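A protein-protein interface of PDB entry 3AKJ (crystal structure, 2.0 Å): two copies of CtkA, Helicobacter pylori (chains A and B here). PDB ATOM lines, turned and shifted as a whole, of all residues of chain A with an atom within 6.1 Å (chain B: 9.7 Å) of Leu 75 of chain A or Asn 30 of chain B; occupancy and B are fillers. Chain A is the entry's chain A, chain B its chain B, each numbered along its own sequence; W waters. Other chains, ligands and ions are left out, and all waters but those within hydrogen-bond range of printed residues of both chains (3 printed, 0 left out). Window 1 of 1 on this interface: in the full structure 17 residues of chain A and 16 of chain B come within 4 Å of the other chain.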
ATOM      1  N   ILE A   4      24.146 -28.434   5.398  1.00  0.00           N
ATOM      2  CA  ILE A   4      23.279 -28.581   6.553  1.00  0.00           C
ATOM      3  C   ILE A   4      22.772 -30.005   6.688  1.00  0.00           C
ATOM      4  O   ILE A   4      22.400 -30.642   5.699  1.00  0.00           O
ATOM      5  CB  ILE A   4      22.070 -27.647   6.480  1.00  0.00           C
ATOM      6  CG1 ILE A   4      22.539 -26.212   6.265  1.00  0.00           C
ATOM      7  CG2 ILE A   4      21.249 -27.747   7.745  1.00  0.00           C
ATOM      8  CD1 ILE A   4      23.768 -25.865   7.071  1.00  0.00           C
ATOM      9  N   PHE A   6      19.782 -32.013   8.752  1.00  0.00           N
ATOM     10  CA  PHE A   6      18.533 -31.757   9.467  1.00  0.00           C
ATOM     11  C   PHE A   6      18.169 -32.910  10.394  1.00  0.00           C
ATOM     12  O   PHE A   6      17.129 -32.889  11.052  1.00  0.00           O
ATOM     13  CB  PHE A   6      17.392 -31.559   8.464  1.00  0.00           C
ATOM     14  CG  PHE A   6      17.556 -30.347   7.570  1.00  0.00           C
ATOM     15  CD1 PHE A   6      17.218 -29.081   8.025  1.00  0.00           C
ATOM     16  CD2 PHE A   6      18.024 -30.479   6.273  1.00  0.00           C
ATOM     17  CE1 PHE A   6      17.367 -27.963   7.213  1.00  0.00           C
ATOM     18  CE2 PHE A   6      18.170 -29.364   5.449  1.00  0.00           C
ATOM     19  CZ  PHE A   6      17.845 -28.106   5.920  1.00  0.00           C
ATOM     20  N   TYR A  29      13.910 -25.396  12.227  1.00  0.00           N
ATOM     21  CA  TYR A  29      15.293 -25.071  11.928  1.00  0.00           C
ATOM     22  C   TYR A  29      15.477 -23.574  12.051  1.00  0.00           C
ATOM     23  O   TYR A  29      14.665 -22.806  11.535  1.00  0.00           O
ATOM     24  CB  TYR A  29      15.680 -25.534  10.523  1.00  0.00           C
ATOM     25  CG  TYR A  29      17.037 -25.022  10.121  1.00  0.00           C
ATOM     26  CD1 TYR A  29      18.198 -25.614  10.610  1.00  0.00           C
ATOM     27  CD2 TYR A  29      17.161 -23.919   9.280  1.00  0.00           C
ATOM     28  CE1 TYR A  29      19.446 -25.131  10.261  1.00  0.00           C
ATOM     29  CE2 TYR A  29      18.401 -23.426   8.929  1.00  0.00           C
ATOM     30  CZ  TYR A  29      19.540 -24.035   9.419  1.00  0.00           C
ATOM     31  OH  TYR A  29      20.775 -23.545   9.057  1.00  0.00           O
ATOM     32  N   TYR A  34      10.146 -25.635   8.816  1.00  0.00           N
ATOM     33  CA  TYR A  34      10.423 -25.992   7.429  1.00  0.00           C
ATOM     34  C   TYR A  34       9.717 -27.293   7.079  1.00  0.00           C
ATOM     35  O   TYR A  34       9.551 -28.179   7.926  1.00  0.00           O
ATOM     36  CB  TYR A  34      11.935 -26.168   7.185  1.00  0.00           C
ATOM     37  CG  TYR A  34      12.731 -24.879   7.191  1.00  0.00           C
ATOM     38  CD1 TYR A  34      13.280 -24.368   6.007  1.00  0.00           C
ATOM     39  CD2 TYR A  34      12.940 -24.172   8.371  1.00  0.00           C
ATOM     40  CE1 TYR A  34      14.016 -23.189   6.007  1.00  0.00           C
ATOM     41  CE2 TYR A  34      13.677 -22.988   8.385  1.00  0.00           C
ATOM     42  CZ  TYR A  34      14.209 -22.502   7.197  1.00  0.00           C
ATOM     43  OH  TYR A  34      14.935 -21.330   7.197  1.00  0.00           O
ATOM     44  N   TYR A  58      15.041 -26.861  -5.432  1.00  0.00           N
ATOM     45  CA  TYR A  58      15.999 -25.909  -4.866  1.00  0.00           C
ATOM     46  C   TYR A  58      16.575 -24.962  -5.922  1.00  0.00           C
ATOM     47  O   TYR A  58      16.578 -23.731  -5.753  1.00  0.00           O
ATOM     48  CB  TYR A  58      17.137 -26.664  -4.169  1.00  0.00           C
ATOM     49  CG  TYR A  58      18.276 -25.771  -3.723  1.00  0.00           C
ATOM     50  CD1 TYR A  58      19.393 -25.575  -4.534  1.00  0.00           C
ATOM     51  CD2 TYR A  58      18.234 -25.129  -2.478  1.00  0.00           C
ATOM     52  CE1 TYR A  58      20.446 -24.751  -4.131  1.00  0.00           C
ATOM     53  CE2 TYR A  58      19.279 -24.310  -2.062  1.00  0.00           C
ATOM     54  CZ  TYR A  58      20.379 -24.121  -2.888  1.00  0.00           C
ATOM     55  OH  TYR A  58      21.401 -23.298  -2.463  1.00  0.00           O
ATOM     56  N   HIS A  62      15.706 -20.908  -6.357  1.00  0.00           N
ATOM     57  CA  HIS A  62      16.806 -19.945  -6.348  1.00  0.00           C
ATOM     58  C   HIS A  62      16.891 -19.143  -7.641  1.00  0.00           C
ATOM     59  O   HIS A  62      17.202 -17.948  -7.625  1.00  0.00           O
ATOM     60  CB  HIS A  62      18.124 -20.631  -5.958  1.00  0.00           C
ATOM     61  CG  HIS A  62      18.227 -20.839  -4.482  1.00  0.00           C
ATOM     62  ND1 HIS A  62      18.749 -19.885  -3.636  1.00  0.00           N
ATOM     63  CD2 HIS A  62      17.773 -21.840  -3.689  1.00  0.00           C
ATOM     64  CE1 HIS A  62      18.656 -20.310  -2.387  1.00  0.00           C
ATOM     65  NE2 HIS A  62      18.063 -21.492  -2.392  1.00  0.00           N
ATOM     66  N   GLU A  73      11.607 -19.790   0.578  1.00  0.00           N
ATOM     67  CA  GLU A  73      13.013 -19.992   0.883  1.00  0.00           C
ATOM     68  C   GLU A  73      13.316 -21.485   0.825  1.00  0.00           C
ATOM     69  O   GLU A  73      12.529 -22.300   1.293  1.00  0.00           O
ATOM     70  CB  GLU A  73      13.347 -19.415   2.269  1.00  0.00           C
ATOM     71  CG  GLU A  73      13.177 -17.900   2.307  1.00  0.00           C
ATOM     72  CD  GLU A  73      13.679 -17.257   3.587  1.00  0.00           C
ATOM     73  OE1 GLU A  73      14.414 -17.920   4.354  1.00  0.00           O
ATOM     74  OE2 GLU A  73      13.337 -16.075   3.813  1.00  0.00           O
ATOM     75  N   THR A  74      14.449 -21.849   0.238  1.00  0.00           N
ATOM     76  CA  THR A  74      14.800 -23.263   0.132  1.00  0.00           C
ATOM     77  C   THR A  74      16.246 -23.532   0.538  1.00  0.00           C
ATOM     78  O   THR A  74      17.126 -22.696   0.334  1.00  0.00           O
ATOM     79  CB  THR A  74      14.553 -23.804  -1.296  1.00  0.00           C
ATOM     80  OG1 THR A  74      15.251 -22.982  -2.239  1.00  0.00           O
ATOM     81  CG2 THR A  74      13.069 -23.763  -1.627  1.00  0.00           C
ATOM     82  N   LEU A  75      16.471 -24.705   1.121  1.00  0.00           N
ATOM     83  CA  LEU A  75      17.806 -25.156   1.507  1.00  0.00           C
ATOM     84  C   LEU A  75      17.928 -26.585   1.056  1.00  0.00           C
ATOM     85  O   LEU A  75      16.956 -27.327   1.111  1.00  0.00           O
ATOM     86  CB  LEU A  75      17.979 -25.125   3.035  1.00  0.00           C
ATOM     87  CG  LEU A  75      17.774 -23.772   3.730  1.00  0.00           C
ATOM     88  CD1 LEU A  75      17.613 -23.922   5.254  1.00  0.00           C
ATOM     89  CD2 LEU A  75      18.934 -22.842   3.390  1.00  0.00           C
ATOM     90  N   LEU A  76      19.117 -26.972   0.612  1.00  0.00           N
ATOM     91  CA  LEU A  76      19.404 -28.373   0.290  1.00  0.00           C
ATOM     92  C   LEU A  76      20.327 -28.903   1.371  1.00  0.00           C
ATOM     93  O   LEU A  76      21.315 -28.265   1.716  1.00  0.00           O
ATOM     94  CB  LEU A  76      20.103 -28.513  -1.069  1.00  0.00           C
ATOM     95  CG  LEU A  76      19.234 -28.720  -2.310  1.00  0.00           C
ATOM     96  CD1 LEU A  76      20.110 -28.797  -3.546  1.00  0.00           C
ATOM     97  CD2 LEU A  76      18.356 -29.969  -2.184  1.00  0.00           C
ATOM     98  N   GLY A  77      20.006 -30.063   1.910  1.00  0.00           N
ATOM     99  CA  GLY A  77      20.825 -30.619   2.963  1.00  0.00           C
ATOM    100  C   GLY A  77      20.612 -32.104   3.021  1.00  0.00           C
ATOM    101  O   GLY A  77      20.168 -32.723   2.053  1.00  0.00           O
ATOM    102  N   VAL A  84      17.761 -33.849   0.905  1.00  0.00           N
ATOM    103  CA  VAL A  84      16.424 -33.295   0.992  1.00  0.00           C
ATOM    104  C   VAL A  84      16.455 -31.824   0.632  1.00  0.00           C
ATOM    105  O   VAL A  84      17.493 -31.166   0.730  1.00  0.00           O
ATOM    106  CB  VAL A  84      15.860 -33.417   2.427  1.00  0.00           C
ATOM    107  CG1 VAL A  84      15.644 -34.873   2.803  1.00  0.00           C
ATOM    108  CG2 VAL A  84      16.795 -32.730   3.423  1.00  0.00           C
ATOM    109  N   VAL A  85      15.310 -31.311   0.203  1.00  0.00           N
ATOM    110  CA  VAL A  85      15.146 -29.879   0.088  1.00  0.00           C
ATOM    111  C   VAL A  85      14.202 -29.422   1.194  1.00  0.00           C
ATOM    112  O   VAL A  85      13.110 -29.971   1.383  1.00  0.00           O
ATOM    113  CB  VAL A  85      14.626 -29.433  -1.303  1.00  0.00           C
ATOM    114  CG1 VAL A  85      13.266 -30.061  -1.606  1.00  0.00           C
ATOM    115  CG2 VAL A  85      14.550 -27.898  -1.369  1.00  0.00           C
ATOM    116  N   ALA A  86      14.643 -28.430   1.951  1.00  0.00           N
ATOM    117  CA  ALA A  86      13.825 -27.886   3.027  1.00  0.00           C
ATOM    118  C   ALA A  86      13.216 -26.565   2.568  1.00  0.00           C
ATOM    119  O   ALA A  86      13.934 -25.661   2.129  1.00  0.00           O
ATOM    120  CB  ALA A  86      14.673 -27.683   4.291  1.00  0.00           C
ATOM    121  N   CYS A  87      11.893 -26.471   2.642  1.00  0.00           N
ATOM    122  CA  CYS A  87      11.186 -25.274   2.210  1.00  0.00           C
ATOM    123  C   CYS A  87      10.590 -24.552   3.423  1.00  0.00           C
ATOM    124  O   CYS A  87       9.832 -25.149   4.193  1.00  0.00           O
ATOM    125  CB  CYS A  87      10.082 -25.658   1.226  1.00  0.00           C
ATOM    126  SG  CYS A  87      10.654 -26.666  -0.170  1.00  0.00           S
ATOM    127  N   ILE A 256      24.441 -20.416  -9.493  1.00  0.00           N
ATOM    128  CA  ILE A 256      23.493 -21.166  -8.680  1.00  0.00           C
ATOM    129  C   ILE A 256      23.673 -22.644  -8.951  1.00  0.00           C
ATOM    130  O   ILE A 256      23.724 -23.466  -8.030  1.00  0.00           O
ATOM    131  CB  ILE A 256      22.011 -20.803  -9.016  1.00  0.00           C
ATOM    132  CG1 ILE A 256      21.689 -19.334  -8.707  1.00  0.00           C
ATOM    133  CG2 ILE A 256      21.057 -21.727  -8.270  1.00  0.00           C
ATOM    134  CD1 ILE A 256      21.810 -18.976  -7.281  1.00  0.00           C
ATOM    135  N   PRO B   2      21.765 -28.697  13.735  1.00  0.00           N
ATOM    136  CA  PRO B   2      22.030 -28.197  12.379  1.00  0.00           C
ATOM    137  C   PRO B   2      22.896 -26.936  12.388  1.00  0.00           C
ATOM    138  O   PRO B   2      22.410 -25.858  12.036  1.00  0.00           O
ATOM    139  CB  PRO B   2      20.629 -27.872  11.842  1.00  0.00           C
ATOM    140  CG  PRO B   2      19.762 -27.742  13.066  1.00  0.00           C
ATOM    141  CD  PRO B   2      20.323 -28.733  14.035  1.00  0.00           C
ATOM    142  N   ILE B   4      26.052 -24.392  11.229  1.00  0.00           N
ATOM    143  CA  ILE B   4      26.632 -24.024   9.944  1.00  0.00           C
ATOM    144  C   ILE B   4      28.065 -23.521  10.074  1.00  0.00           C
ATOM    145  O   ILE B   4      28.325 -22.509  10.723  1.00  0.00           O
ATOM    146  CB  ILE B   4      25.801 -22.947   9.215  1.00  0.00           C
ATOM    147  CG1 ILE B   4      24.339 -23.381   9.076  1.00  0.00           C
ATOM    148  CG2 ILE B   4      26.403 -22.659   7.845  1.00  0.00           C
ATOM    149  CD1 ILE B   4      23.529 -23.307  10.367  1.00  0.00           C
ATOM    150  N   ASP B   5      28.993 -24.238   9.452  1.00  0.00           N
ATOM    151  CA  ASP B   5      30.371 -23.783   9.369  1.00  0.00           C
ATOM    152  C   ASP B   5      30.557 -22.889   8.147  1.00  0.00           C
ATOM    153  O   ASP B   5      30.438 -23.344   7.011  1.00  0.00           O
ATOM    154  CB  ASP B   5      31.328 -24.969   9.284  1.00  0.00           C
ATOM    155  CG  ASP B   5      32.768 -24.535   9.143  1.00  0.00           C
ATOM    156  OD1 ASP B   5      33.109 -23.449   9.663  1.00  0.00           O
ATOM    157  OD2 ASP B   5      33.555 -25.271   8.508  1.00  0.00           O
ATOM    158  N   PHE B   6      30.854 -21.618   8.384  1.00  0.00           N
ATOM    159  CA  PHE B   6      31.004 -20.664   7.292  1.00  0.00           C
ATOM    160  C   PHE B   6      32.445 -20.573   6.800  1.00  0.00           C
ATOM    161  O   PHE B   6      32.724 -19.916   5.792  1.00  0.00           O
ATOM    162  CB  PHE B   6      30.514 -19.282   7.723  1.00  0.00           C
ATOM    163  CG  PHE B   6      29.066 -19.251   8.110  1.00  0.00           C
ATOM    164  CD1 PHE B   6      28.078 -19.237   7.139  1.00  0.00           C
ATOM    165  CD2 PHE B   6      28.693 -19.239   9.442  1.00  0.00           C
ATOM    166  CE1 PHE B   6      26.742 -19.211   7.489  1.00  0.00           C
ATOM    167  CE2 PHE B   6      27.357 -19.212   9.800  1.00  0.00           C
ATOM    168  CZ  PHE B   6      26.381 -19.198   8.823  1.00  0.00           C
ATOM    169  N   CYS B   9      32.890 -20.943   3.069  1.00  0.00           N
ATOM    170  CA  CYS B   9      32.099 -20.135   2.145  1.00  0.00           C
ATOM    171  C   CYS B   9      32.947 -19.158   1.337  1.00  0.00           C
ATOM    172  O   CYS B   9      33.975 -18.668   1.809  1.00  0.00           O
ATOM    173  CB  CYS B   9      30.998 -19.383   2.893  1.00  0.00           C
ATOM    174  SG  CYS B   9      29.747 -20.471   3.574  1.00  0.00           S
ATOM    175  N   GLU B  10      32.495 -18.880   0.117  1.00  0.00           N
ATOM    176  CA  GLU B  10      33.195 -17.977  -0.789  1.00  0.00           C
ATOM    177  C   GLU B  10      33.078 -16.531  -0.331  1.00  0.00           C
ATOM    178  O   GLU B  10      31.975 -15.998  -0.205  1.00  0.00           O
ATOM    179  CB  GLU B  10      32.641 -18.111  -2.208  1.00  0.00           C
ATOM    180  CG  GLU B  10      33.104 -17.015  -3.147  1.00  0.00           C
ATOM    181  CD  GLU B  10      32.351 -17.017  -4.464  1.00  0.00           C
ATOM    182  OE1 GLU B  10      32.421 -18.032  -5.193  1.00  0.00           O
ATOM    183  OE2 GLU B  10      31.694 -15.999  -4.773  1.00  0.00           O
ATOM    184  N   LEU B  27      30.465 -12.803   2.765  1.00  0.00           N
ATOM    185  CA  LEU B  27      30.560 -14.073   2.045  1.00  0.00           C
ATOM    186  C   LEU B  27      29.234 -14.561   1.451  1.00  0.00           C
ATOM    187  O   LEU B  27      28.152 -14.089   1.817  1.00  0.00           O
ATOM    188  CB  LEU B  27      31.203 -15.160   2.920  1.00  0.00           C
ATOM    189  CG  LEU B  27      30.626 -15.468   4.302  1.00  0.00           C
ATOM    190  CD1 LEU B  27      29.181 -15.948   4.220  1.00  0.00           C
ATOM    191  CD2 LEU B  27      31.495 -16.505   4.997  1.00  0.00           C
ATOM    192  N   PHE B  28      29.331 -15.504   0.520  1.00  0.00           N
ATOM    193  CA  PHE B  28      28.143 -16.094  -0.076  1.00  0.00           C
ATOM    194  C   PHE B  28      27.754 -17.364   0.655  1.00  0.00           C
ATOM    195  O   PHE B  28      28.591 -18.216   0.929  1.00  0.00           O
ATOM    196  CB  PHE B  28      28.359 -16.397  -1.559  1.00  0.00           C
ATOM    197  CG  PHE B  28      28.466 -15.172  -2.418  1.00  0.00           C
ATOM    198  CD1 PHE B  28      27.326 -14.548  -2.900  1.00  0.00           C
ATOM    199  CD2 PHE B  28      29.708 -14.643  -2.747  1.00  0.00           C
ATOM    200  CE1 PHE B  28      27.418 -13.421  -3.692  1.00  0.00           C
ATOM    201  CE2 PHE B  28      29.809 -13.515  -3.538  1.00  0.00           C
ATOM    202  CZ  PHE B  28      28.661 -12.903  -4.012  1.00  0.00           C
ATOM    203  N   TYR B  29      26.475 -17.472   0.980  1.00  0.00           N
ATOM    204  CA  TYR B  29      25.932 -18.687   1.558  1.00  0.00           C
ATOM    205  C   TYR B  29      24.537 -18.927   0.997  1.00  0.00           C
ATOM    206  O   TYR B  29      23.712 -18.017   0.958  1.00  0.00           O
ATOM    207  CB  TYR B  29      25.882 -18.585   3.081  1.00  0.00           C
ATOM    208  CG  TYR B  29      25.034 -19.655   3.714  1.00  0.00           C
ATOM    209  CD1 TYR B  29      25.525 -20.946   3.903  1.00  0.00           C
ATOM    210  CD2 TYR B  29      23.735 -19.379   4.115  1.00  0.00           C
ATOM    211  CE1 TYR B  29      24.737 -21.932   4.481  1.00  0.00           C
ATOM    212  CE2 TYR B  29      22.943 -20.352   4.694  1.00  0.00           C
ATOM    213  CZ  TYR B  29      23.441 -21.621   4.877  1.00  0.00           C
ATOM    214  OH  TYR B  29      22.633 -22.573   5.454  1.00  0.00           O
ATOM    215  N   ASN B  30      24.280 -20.148   0.549  1.00  0.00           N
ATOM    216  CA  ASN B  30      23.009 -20.452  -0.091  1.00  0.00           C
ATOM    217  C   ASN B  30      22.715 -19.480  -1.227  1.00  0.00           C
ATOM    218  O   ASN B  30      21.580 -19.030  -1.392  1.00  0.00           O
ATOM    219  CB  ASN B  30      21.875 -20.408   0.937  1.00  0.00           C
ATOM    220  CG  ASN B  30      20.684 -21.252   0.529  1.00  0.00           C
ATOM    221  OD1 ASN B  30      20.835 -22.308  -0.096  1.00  0.00           O
ATOM    222  ND2 ASN B  30      19.493 -20.796   0.885  1.00  0.00           N
ATOM    223  N   ASN B  31      23.751 -19.128  -1.988  1.00  0.00           N
ATOM    224  CA  ASN B  31      23.577 -18.264  -3.156  1.00  0.00           C
ATOM    225  C   ASN B  31      23.311 -16.806  -2.836  1.00  0.00           C
ATOM    226  O   ASN B  31      22.997 -16.023  -3.733  1.00  0.00           O
ATOM    227  CB  ASN B  31      22.430 -18.780  -4.021  1.00  0.00           C
ATOM    228  CG  ASN B  31      22.700 -20.152  -4.563  1.00  0.00           C
ATOM    229  OD1 ASN B  31      23.764 -20.406  -5.133  1.00  0.00           O
ATOM    230  ND2 ASN B  31      21.741 -21.055  -4.385  1.00  0.00           N
ATOM    231  N   GLU B  32      23.417 -16.439  -1.564  1.00  0.00           N
ATOM    232  CA  GLU B  32      23.153 -15.056  -1.184  1.00  0.00           C
ATOM    233  C   GLU B  32      24.248 -14.489  -0.283  1.00  0.00           C
ATOM    234  O   GLU B  32      24.979 -15.233   0.370  1.00  0.00           O
ATOM    235  CB  GLU B  32      21.768 -14.939  -0.542  1.00  0.00           C
ATOM    236  CG  GLU B  32      20.675 -15.550  -1.407  1.00  0.00           C
ATOM    237  CD  GLU B  32      19.290 -15.385  -0.804  1.00  0.00           C
ATOM    238  OE1 GLU B  32      18.992 -16.063   0.212  1.00  0.00           O
ATOM    239  OE2 GLU B  32      18.507 -14.575  -1.355  1.00  0.00           O
ATOM    240  N   LEU B  33      24.366 -13.167  -0.277  1.00  0.00           N
ATOM    241  CA  LEU B  33      25.425 -12.483   0.455  1.00  0.00           C
ATOM    242  C   LEU B  33      25.035 -12.329   1.919  1.00  0.00           C
ATOM    243  O   LEU B  33      23.942 -11.854   2.213  1.00  0.00           O
ATOM    244  CB  LEU B  33      25.659 -11.101  -0.158  1.00  0.00           C
ATOM    245  CG  LEU B  33      27.096 -10.588  -0.264  1.00  0.00           C
ATOM    246  CD1 LEU B  33      27.996 -11.652  -0.866  1.00  0.00           C
ATOM    247  CD2 LEU B  33      27.144  -9.314  -1.100  1.00  0.00           C
ATOM    248  N   TYR B  34      25.921 -12.752   2.818  1.00  0.00           N
ATOM    249  CA  TYR B  34      25.753 -12.533   4.250  1.00  0.00           C
ATOM    250  C   TYR B  34      26.955 -11.780   4.789  1.00  0.00           C
ATOM    251  O   TYR B  34      28.092 -12.075   4.425  1.00  0.00           O
ATOM    252  CB  TYR B  34      25.647 -13.862   4.999  1.00  0.00           C
ATOM    253  CG  TYR B  34      24.351 -14.604   4.792  1.00  0.00           C
ATOM    254  CD1 TYR B  34      23.442 -14.757   5.833  1.00  0.00           C
ATOM    255  CD2 TYR B  34      24.038 -15.158   3.557  1.00  0.00           C
ATOM    256  CE1 TYR B  34      22.258 -15.438   5.648  1.00  0.00           C
ATOM    257  CE2 TYR B  34      22.859 -15.840   3.363  1.00  0.00           C
ATOM    258  CZ  TYR B  34      21.973 -15.980   4.410  1.00  0.00           C
ATOM    259  OH  TYR B  34      20.795 -16.659   4.210  1.00  0.00           O
ATOM    260  N   GLU B  73      17.601 -11.343   8.289  1.00  0.00           N
ATOM    261  CA  GLU B  73      17.776 -12.752   8.564  1.00  0.00           C
ATOM    262  C   GLU B  73      19.091 -12.985   9.291  1.00  0.00           C
ATOM    263  O   GLU B  73      20.131 -12.446   8.913  1.00  0.00           O
ATOM    264  CB  GLU B  73      17.753 -13.555   7.261  1.00  0.00           C
ATOM    265  CG  GLU B  73      18.210 -14.999   7.460  1.00  0.00           C
ATOM    266  CD  GLU B  73      18.177 -15.820   6.171  1.00  0.00           C
ATOM    267  OE1 GLU B  73      17.465 -15.409   5.227  1.00  0.00           O
ATOM    268  OE2 GLU B  73      18.854 -16.871   6.118  1.00  0.00           O
ATOM    269  N   LEU B  75      21.743 -15.979  11.344  1.00  0.00           N
ATOM    270  CA  LEU B  75      22.123 -17.358  11.595  1.00  0.00           C
ATOM    271  C   LEU B  75      23.273 -17.351  12.569  1.00  0.00           C
ATOM    272  O   LEU B  75      24.124 -16.470  12.515  1.00  0.00           O
ATOM    273  CB  LEU B  75      22.606 -18.033  10.309  1.00  0.00           C
ATOM    274  CG  LEU B  75      21.677 -18.051   9.095  1.00  0.00           C
ATOM    275  CD1 LEU B  75      22.459 -18.433   7.841  1.00  0.00           C
ATOM    276  CD2 LEU B  75      20.507 -19.006   9.326  1.00  0.00           C
ATOM    277  N   LYS B  88      21.975 -11.728   6.727  1.00  0.00           N
ATOM    278  CA  LYS B  88      21.704 -11.714   5.290  1.00  0.00           C
ATOM    279  C   LYS B  88      21.569 -10.292   4.783  1.00  0.00           C
ATOM    280  O   LYS B  88      20.791  -9.502   5.320  1.00  0.00           O
ATOM    281  CB  LYS B  88      20.444 -12.521   4.965  1.00  0.00           C
ATOM    282  CG  LYS B  88      20.171 -12.762   3.472  1.00  0.00           C
ATOM    283  CD  LYS B  88      18.727 -13.272   3.263  1.00  0.00           C
ATOM    284  CE  LYS B  88      18.395 -13.480   1.791  1.00  0.00           C
ATOM    285  NZ  LYS B  88      17.046 -14.104   1.591  1.00  0.00           N
HETATM  286  O   HOH W   1      23.373 -23.284  -5.359  1.00  0.00           O
HETATM  287  O   HOH W   2      15.349 -14.202   4.693  1.00  0.00           O
HETATM  288  O   HOH W   3      21.262 -24.956   0.807  1.00  0.00           O
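Ile 4 of chain B touches its own counterpart, Ile 4 of chain A.
Ile 4 of chain A touches Tyr 29 of chain B, and with the chains exchanged Tyr 29 of chain A touches Ile 4 of chain B.
6 positions are printed for both chains.
OD1 of Asn 30 of chain B lies within hydrogen-bond range of OH of Tyr 58 of chain A (2.6 Å).
The side-chain hydroxyl of Tyr 58 of chain A lies within hydrogen-bond range of the side-chain amide nitrogen of Asn 31 of chain B.
ND2 of Asn 31 of chain B lies within hydrogen-bond range of ND1 of His 62 of chain A, at 3.3 Å.
ND2 of Asn 30 of chain B is in hydrogen-bond range of O of Thr 74 of chain A (3.1 Å).
Water W2 lies within hydrogen-bond range of the side-chain carboxylate (OE1) of Glu 73 of chain B (2.5 Å) and the side-chain carboxylate (OE2) of Glu 73 of chain A (2.9 Å).
Water W1 lies within hydrogen-bond range of the backbone carbonyl oxygen of Ile 256 of chain A (2.7 Å) and the side-chain amide oxygen of Asn 31 of chain B (2.9 Å).
Water W3 lies within hydrogen-bond range of OD1 of Asn 30 of chain B (2.8 Å) and N of Leu 76 of chain A (3.0 Å).
Of chain B, only Asn 30 (3.3 Å) comes within 4 Å of Leu 75 of chain A.
Asn 30 of chain B touches just these residues of chain A: Tyr 58 (2.6 Å), His 62 (3.3 Å), Thr 74 (3.1 Å) and Leu 75 (3.3 Å).
Of the printed residues of chain B, Tyr 58 of chain A touches Asn 30 (2.6 Å) and Asn 31 (3.0 Å).
Printed residues of chain B within 4 Å of Tyr 29 of chain A: Pro 2 (3.4 Å) and Ile 4 (3.1 Å).
Of the printed residues of chain B, His 62 of chain A touches Asn 30 and Asn 31.
Of the printed residues of chain A, Asn 31 of chain B touches Tyr 58, His 62 and Ile 256.
Printed residues of chain B within 4 Å of Ile 256 of chain A: Asn 31 (3.1 Å).
Tyr 34 of chain B touches none of the printed residues of chain A.
The nearest residue of chain B that does not touch Leu 75 of chain A is Tyr 29 of chain B (4.2 Å).
The nearest residue of chain A that does not touch Asn 30 of chain B is Leu 76 of chain A (5.0 Å).
A ring nitrogen (NE2) of His 62 of chain A lies within hydrogen-bond range of the backbone carbonyl oxygen (O) of Thr 74 of chain A, at 3.1 Å.
The backbone NH (N) of Ala 86 of chain A lies within hydrogen-bond range of the backbone carbonyl oxygen (O) of Leu 75 of chain A.
Of the 17 printed residues of chain B, 5 touch a printed residue of chain A.
Hydrophobic or aromatic side chains of chain B that line the printed part of chain A: Pro 2, Ile 4 and Tyr 29.
Along chain B the printed residues that touch a printed residue of chain A span positions 2 to 31.
Among the printed residues, no Asp or Glu carboxylate lies within 4 Å of a Lys or Arg side-chain nitrogen of the other chain.
Ile 4 of chain B touches Ile 4 of chain A (CG1 to CD1, 3.2 Å).
Tyr 29 of chain B touches Ile 4 of chain A (OH to CG1, 3.7 Å).
CE1 of Tyr 29 of chain A touches CB of Pro 2 of chain B, 3.4 Å away.
Tyr 29 of chain A touches Ile 4 of chain B.
O of Asn 30 of chain B touches CE1 of His 62 of chain A, at 3.3 Å.
CD2 of Leu 75 of chain A touches ND2 of Asn 30 of chain B, at 3.3 Å.
Ile 256 of chain A touches Asn 31 of chain B.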
